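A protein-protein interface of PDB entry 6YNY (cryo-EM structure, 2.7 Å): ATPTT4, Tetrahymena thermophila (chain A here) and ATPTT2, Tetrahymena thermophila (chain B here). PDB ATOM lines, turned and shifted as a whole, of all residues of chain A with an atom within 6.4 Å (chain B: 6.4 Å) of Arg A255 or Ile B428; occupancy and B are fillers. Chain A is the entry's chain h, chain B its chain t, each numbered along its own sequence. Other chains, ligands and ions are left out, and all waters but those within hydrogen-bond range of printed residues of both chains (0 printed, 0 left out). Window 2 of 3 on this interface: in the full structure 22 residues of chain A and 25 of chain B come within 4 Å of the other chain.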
ATOM      1  N   GLU A 253      15.179 -13.533  -9.770  1.00  0.00           N
ATOM      2  CA  GLU A 253      16.047 -12.481 -10.278  1.00  0.00           C
ATOM      3  C   GLU A 253      15.829 -12.281 -11.770  1.00  0.00           C
ATOM      4  O   GLU A 253      15.925 -13.224 -12.559  1.00  0.00           O
ATOM      5  CB  GLU A 253      17.509 -12.811  -9.988  1.00  0.00           C
ATOM      6  CG  GLU A 253      18.490 -11.801 -10.542  1.00  0.00           C
ATOM      7  CD  GLU A 253      19.888 -11.967  -9.995  1.00  0.00           C
ATOM      8  OE1 GLU A 253      20.027 -12.279  -8.794  1.00  0.00           O
ATOM      9  OE2 GLU A 253      20.853 -11.782 -10.764  1.00  0.00           O
ATOM     10  N   GLN A 254      15.533 -11.044 -12.152  1.00  0.00           N
ATOM     11  CA  GLN A 254      15.304 -10.680 -13.539  1.00  0.00           C
ATOM     12  C   GLN A 254      16.328  -9.640 -13.965  1.00  0.00           C
ATOM     13  O   GLN A 254      16.986  -9.005 -13.138  1.00  0.00           O
ATOM     14  CB  GLN A 254      13.890 -10.128 -13.754  1.00  0.00           C
ATOM     15  CG  GLN A 254      12.790 -11.126 -13.495  1.00  0.00           C
ATOM     16  CD  GLN A 254      12.838 -12.302 -14.442  1.00  0.00           C
ATOM     17  OE1 GLN A 254      13.477 -12.245 -15.491  1.00  0.00           O
ATOM     18  NE2 GLN A 254      12.162 -13.380 -14.073  1.00  0.00           N
ATOM     19  N   ARG A 255      16.447  -9.470 -15.276  1.00  0.00           N
ATOM     20  CA  ARG A 255      17.408  -8.550 -15.856  1.00  0.00           C
ATOM     21  C   ARG A 255      16.736  -7.761 -16.968  1.00  0.00           C
ATOM     22  O   ARG A 255      15.792  -8.236 -17.602  1.00  0.00           O
ATOM     23  CB  ARG A 255      18.623  -9.304 -16.402  1.00  0.00           C
ATOM     24  CG  ARG A 255      19.777  -8.419 -16.810  1.00  0.00           C
ATOM     25  CD  ARG A 255      20.526  -8.988 -17.991  1.00  0.00           C
ATOM     26  NE  ARG A 255      21.656  -9.822 -17.610  1.00  0.00           N
ATOM     27  CZ  ARG A 255      22.909  -9.392 -17.524  1.00  0.00           C
ATOM     28  NH1 ARG A 255      23.212  -8.130 -17.787  1.00  0.00           N
ATOM     29  NH2 ARG A 255      23.867 -10.231 -17.176  1.00  0.00           N
ATOM     30  N   ARG A 256      17.218  -6.542 -17.185  1.00  0.00           N
ATOM     31  CA  ARG A 256      16.713  -5.739 -18.280  1.00  0.00           C
ATOM     32  C   ARG A 256      17.020  -6.428 -19.609  1.00  0.00           C
ATOM     33  O   ARG A 256      18.056  -7.082 -19.751  1.00  0.00           O
ATOM     34  CB  ARG A 256      17.333  -4.349 -18.274  1.00  0.00           C
ATOM     35  CG  ARG A 256      16.920  -3.469 -17.126  1.00  0.00           C
ATOM     36  CD  ARG A 256      17.377  -2.051 -17.367  1.00  0.00           C
ATOM     37  NE  ARG A 256      17.030  -1.143 -16.282  1.00  0.00           N
ATOM     38  CZ  ARG A 256      15.870  -0.507 -16.176  1.00  0.00           C
ATOM     39  NH1 ARG A 256      14.920  -0.677 -17.082  1.00  0.00           N
ATOM     40  NH2 ARG A 256      15.660   0.301 -15.152  1.00  0.00           N
ATOM     41  N   PRO A 257      16.141  -6.302 -20.595  1.00  0.00           N
ATOM     42  CA  PRO A 257      16.422  -6.903 -21.898  1.00  0.00           C
ATOM     43  C   PRO A 257      17.550  -6.181 -22.612  1.00  0.00           C
ATOM     44  O   PRO A 257      17.795  -4.991 -22.398  1.00  0.00           O
ATOM     45  CB  PRO A 257      15.098  -6.752 -22.651  1.00  0.00           C
ATOM     46  CG  PRO A 257      14.442  -5.619 -22.020  1.00  0.00           C
ATOM     47  CD  PRO A 257      14.833  -5.630 -20.582  1.00  0.00           C
ATOM     48  N   PHE A 258      18.245  -6.926 -23.471  1.00  0.00           N
ATOM     49  CA  PHE A 258      19.363  -6.354 -24.207  1.00  0.00           C
ATOM     50  C   PHE A 258      18.941  -5.127 -25.000  1.00  0.00           C
ATOM     51  O   PHE A 258      19.733  -4.193 -25.166  1.00  0.00           O
ATOM     52  CB  PHE A 258      19.955  -7.415 -25.130  1.00  0.00           C
ATOM     53  CG  PHE A 258      21.205  -6.987 -25.831  1.00  0.00           C
ATOM     54  CD1 PHE A 258      22.438  -7.157 -25.236  1.00  0.00           C
ATOM     55  CD2 PHE A 258      21.149  -6.430 -27.091  1.00  0.00           C
ATOM     56  CE1 PHE A 258      23.586  -6.769 -25.880  1.00  0.00           C
ATOM     57  CE2 PHE A 258      22.293  -6.042 -27.737  1.00  0.00           C
ATOM     58  CZ  PHE A 258      23.514  -6.212 -27.132  1.00  0.00           C
ATOM     59  N   HIS A 268      26.570  -0.640 -13.067  1.00  0.00           N
ATOM     60  CA  HIS A 268      27.600  -1.252 -12.242  1.00  0.00           C
ATOM     61  C   HIS A 268      28.843  -0.370 -12.191  1.00  0.00           C
ATOM     62  O   HIS A 268      29.967  -0.862 -12.267  1.00  0.00           O
ATOM     63  CB  HIS A 268      27.947  -2.641 -12.775  1.00  0.00           C
ATOM     64  CG  HIS A 268      28.528  -2.632 -14.154  1.00  0.00           C
ATOM     65  ND1 HIS A 268      27.764  -2.426 -15.282  1.00  0.00           N
ATOM     66  CD2 HIS A 268      29.797  -2.806 -14.588  1.00  0.00           C
ATOM     67  CE1 HIS A 268      28.537  -2.473 -16.350  1.00  0.00           C
ATOM     68  NE2 HIS A 268      29.776  -2.703 -15.957  1.00  0.00           N
ATOM     69  N   MET B 414      15.408  -1.954 -10.774  1.00  0.00           N
ATOM     70  CA  MET B 414      16.597  -2.769 -10.953  1.00  0.00           C
ATOM     71  C   MET B 414      17.722  -2.223 -10.091  1.00  0.00           C
ATOM     72  O   MET B 414      17.993  -1.018 -10.103  1.00  0.00           O
ATOM     73  CB  MET B 414      17.012  -2.802 -12.422  1.00  0.00           C
ATOM     74  CG  MET B 414      16.038  -3.527 -13.316  1.00  0.00           C
ATOM     75  SD  MET B 414      16.105  -5.307 -13.131  1.00  0.00           S
ATOM     76  CE  MET B 414      14.851  -5.785 -14.303  1.00  0.00           C
ATOM     77  N   ARG B 422      29.626 -12.533  -9.679  1.00  0.00           N
ATOM     78  CA  ARG B 422      28.987 -13.745 -10.155  1.00  0.00           C
ATOM     79  C   ARG B 422      30.039 -14.722 -10.657  1.00  0.00           C
ATOM     80  O   ARG B 422      31.103 -14.326 -11.140  1.00  0.00           O
ATOM     81  CB  ARG B 422      27.981 -13.437 -11.262  1.00  0.00           C
ATOM     82  CG  ARG B 422      26.802 -12.610 -10.789  1.00  0.00           C
ATOM     83  CD  ARG B 422      25.609 -12.793 -11.687  1.00  0.00           C
ATOM     84  NE  ARG B 422      24.386 -12.247 -11.108  1.00  0.00           N
ATOM     85  CZ  ARG B 422      24.055 -10.962 -11.131  1.00  0.00           C
ATOM     86  NH1 ARG B 422      24.854 -10.074 -11.698  1.00  0.00           N
ATOM     87  NH2 ARG B 422      22.920 -10.567 -10.585  1.00  0.00           N
ATOM     88  N   SER B 425      31.818 -16.333 -15.935  1.00  0.00           N
ATOM     89  CA  SER B 425      32.804 -15.395 -16.456  1.00  0.00           C
ATOM     90  C   SER B 425      32.284 -14.662 -17.683  1.00  0.00           C
ATOM     91  O   SER B 425      32.632 -13.497 -17.895  1.00  0.00           O
ATOM     92  CB  SER B 425      34.102 -16.127 -16.789  1.00  0.00           C
ATOM     93  OG  SER B 425      34.673 -16.698 -15.626  1.00  0.00           O
ATOM     94  N   LYS B 426      31.467 -15.322 -18.497  1.00  0.00           N
ATOM     95  CA  LYS B 426      30.890 -14.703 -19.688  1.00  0.00           C
ATOM     96  C   LYS B 426      29.556 -14.046 -19.354  1.00  0.00           C
ATOM     97  O   LYS B 426      28.540 -14.262 -20.013  1.00  0.00           O
ATOM     98  CB  LYS B 426      30.729 -15.745 -20.787  1.00  0.00           C
ATOM     99  CG  LYS B 426      31.997 -16.511 -21.096  1.00  0.00           C
ATOM    100  CD  LYS B 426      31.931 -17.179 -22.457  1.00  0.00           C
ATOM    101  CE  LYS B 426      30.785 -18.163 -22.554  1.00  0.00           C
ATOM    102  NZ  LYS B 426      30.754 -18.822 -23.888  1.00  0.00           N
ATOM    103  N   HIS B 427      29.571 -13.213 -18.318  1.00  0.00           N
ATOM    104  CA  HIS B 427      28.383 -12.545 -17.805  1.00  0.00           C
ATOM    105  C   HIS B 427      28.535 -11.048 -18.007  1.00  0.00           C
ATOM    106  O   HIS B 427      29.521 -10.456 -17.558  1.00  0.00           O
ATOM    107  CB  HIS B 427      28.179 -12.871 -16.325  1.00  0.00           C
ATOM    108  CG  HIS B 427      26.960 -12.245 -15.727  1.00  0.00           C
ATOM    109  ND1 HIS B 427      26.978 -11.002 -15.135  1.00  0.00           N
ATOM    110  CD2 HIS B 427      25.688 -12.692 -15.621  1.00  0.00           C
ATOM    111  CE1 HIS B 427      25.768 -10.708 -14.696  1.00  0.00           C
ATOM    112  NE2 HIS B 427      24.966 -11.718 -14.976  1.00  0.00           N
ATOM    113  N   ILE B 428      27.567 -10.442 -18.684  1.00  0.00           N
ATOM    114  CA  ILE B 428      27.553  -9.002 -18.904  1.00  0.00           C
ATOM    115  C   ILE B 428      26.912  -8.364 -17.679  1.00  0.00           C
ATOM    116  O   ILE B 428      25.701  -8.467 -17.474  1.00  0.00           O
ATOM    117  CB  ILE B 428      26.803  -8.632 -20.187  1.00  0.00           C
ATOM    118  CG1 ILE B 428      27.504  -9.251 -21.396  1.00  0.00           C
ATOM    119  CG2 ILE B 428      26.716  -7.124 -20.338  1.00  0.00           C
ATOM    120  CD1 ILE B 428      26.886  -8.899 -22.727  1.00  0.00           C
ATOM    121  N   TYR B 429      27.730  -7.710 -16.863  1.00  0.00           N
ATOM    122  CA  TYR B 429      27.239  -7.141 -15.620  1.00  0.00           C
ATOM    123  C   TYR B 429      26.275  -6.000 -15.896  1.00  0.00           C
ATOM    124  O   TYR B 429      26.515  -5.152 -16.758  1.00  0.00           O
ATOM    125  CB  TYR B 429      28.403  -6.656 -14.763  1.00  0.00           C
ATOM    126  CG  TYR B 429      29.059  -7.768 -13.990  1.00  0.00           C
ATOM    127  CD1 TYR B 429      28.591  -8.133 -12.742  1.00  0.00           C
ATOM    128  CD2 TYR B 429      30.136  -8.461 -14.512  1.00  0.00           C
ATOM    129  CE1 TYR B 429      29.176  -9.147 -12.033  1.00  0.00           C
ATOM    130  CE2 TYR B 429      30.729  -9.482 -13.808  1.00  0.00           C
ATOM    131  CZ  TYR B 429      30.243  -9.822 -12.568  1.00  0.00           C
ATOM    132  OH  TYR B 429      30.830 -10.838 -11.859  1.00  0.00           O
ATOM    133  N   GLY B 430      25.170  -5.994 -15.160  1.00  0.00           N
ATOM    134  CA  GLY B 430      24.151  -4.983 -15.330  1.00  0.00           C
ATOM    135  C   GLY B 430      23.235  -4.968 -14.130  1.00  0.00           C
ATOM    136  O   GLY B 430      23.407  -5.727 -13.174  1.00  0.00           O
ATOM    137  N   ASP B 431      22.252  -4.080 -14.192  1.00  0.00           N
ATOM    138  CA  ASP B 431      21.288  -3.960 -13.114  1.00  0.00           C
ATOM    139  C   ASP B 431      20.321  -5.137 -13.140  1.00  0.00           C
ATOM    140  O   ASP B 431      20.023  -5.705 -14.194  1.00  0.00           O
ATOM    141  CB  ASP B 431      20.527  -2.640 -13.225  1.00  0.00           C
ATOM    142  CG  ASP B 431      19.761  -2.511 -14.523  1.00  0.00           C
ATOM    143  OD1 ASP B 431      19.917  -3.384 -15.402  1.00  0.00           O
ATOM    144  OD2 ASP B 431      19.002  -1.532 -14.665  1.00  0.00           O
ATOM    145  N   TYR B 432      19.840  -5.511 -11.960  1.00  0.00           N
ATOM    146  CA  TYR B 432      18.957  -6.655 -11.817  1.00  0.00           C
ATOM    147  C   TYR B 432      17.927  -6.372 -10.738  1.00  0.00           C
ATOM    148  O   TYR B 432      18.150  -5.560  -9.839  1.00  0.00           O
ATOM    149  CB  TYR B 432      19.730  -7.927 -11.459  1.00  0.00           C
ATOM    150  CG  TYR B 432      20.407  -7.873 -10.112  1.00  0.00           C
ATOM    151  CD1 TYR B 432      19.794  -8.397  -8.988  1.00  0.00           C
ATOM    152  CD2 TYR B 432      21.658  -7.303  -9.965  1.00  0.00           C
ATOM    153  CE1 TYR B 432      20.405  -8.351  -7.760  1.00  0.00           C
ATOM    154  CE2 TYR B 432      22.275  -7.252  -8.740  1.00  0.00           C
ATOM    155  CZ  TYR B 432      21.646  -7.779  -7.640  1.00  0.00           C
ATOM    156  OH  TYR B 432      22.260  -7.733  -6.411  1.00  0.00           O
ATOM    157  N   SER B 433      16.791  -7.050 -10.849  1.00  0.00           N
ATOM    158  CA  SER B 433      15.790  -7.032  -9.798  1.00  0.00           C
ATOM    159  C   SER B 433      16.050  -8.189  -8.844  1.00  0.00           C
ATOM    160  O   SER B 433      16.066  -9.344  -9.284  1.00  0.00           O
ATOM    161  CB  SER B 433      14.397  -7.146 -10.387  1.00  0.00           C
ATOM    162  OG  SER B 433      14.211  -8.394 -11.016  1.00  0.00           O
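Among the printed residues, merely in contact across the chains: Glu A253 with Ser B433 (3.3 Å), Gln A254 with Tyr B432 (3.3 Å), Glu A253 with Tyr B432 (3.7 Å), Arg A255 with Asp B431 (3.8 Å), Gln A254 with Met B414 (3.8 Å), Arg A256 with Met B414 (3.8 Å), Arg A255 with Met B414 (3.8 Å) and Arg A255 with Gly B430 (3.9 Å).
SD of Met B414 sits at hydrogen-bond distance from N of Ser B433, at 3.0 Å.
The backbone NH of Arg B422 is in hydrogen-bond range of the side-chain hydroxyl of Tyr B429 (3.0 Å).
Hydrophobic or aromatic side chains of chain A within 4 Å of the printed part of chain B: His A268.
Of the 11 printed residues of chain B, 9 touch a printed residue of chain A.
Along chain B the printed residues that touch a printed residue of chain A span positions 414 to 433.
Among the printed residues, 14 pairs touch across the chains.
Among the printed residues, Asp or Glu carboxylates within 4 Å of a Lys or Arg side-chain nitrogen of the other chain: Glu A253 with Arg B422 (2.4 Å) and Arg A256 with Asp B431 (2.6 Å).
The side-chain carboxylate of Glu A253 is in salt-bridge range of the guanidinium group of Arg B422.
The guanidinium group (NH2) of Arg A255 sits at hydrogen-bond distance from a ring nitrogen (NE2) of His B427 (2.9 Å).
The backbone carbonyl oxygen (O) of Ile B428 lies within hydrogen-bond range of the guanidinium group (NH1) of Arg A255, 2.5 Å away.
O of Tyr B429 sits at hydrogen-bond distance from ND1 of His A268.
The guanidinium group of Arg A256 lies within salt-bridge range of the side-chain carboxylate of Asp B431, 2.6 Å away.
O of Gln A254 lies within hydrogen-bond range of N of Ser B433 (3.0 Å).
Of chain B, only Met B414, His B427, Ile B428, Gly B430 and Asp B431 come within 4 Å of Arg A255.
Of chain A, only Arg A255 (2.5 Å) comes within 4 Å of Ile B428.
Of the printed residues of chain A, Gly B430 touches Arg A255 (3.9 Å).
Printed residues of chain A within 4 Å of Ser B433: Glu A253 and Gln A254.
Printed residues of chain B within 4 Å of Glu A253: Arg B422, Tyr B432 and Ser B433.
The nearest residue of chain B that does not touch Arg A255 is Tyr B429 (4.2 Å).
The nearest printed residue of chain A that does not touch His B427 is Glu A253 (5.9 Å).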
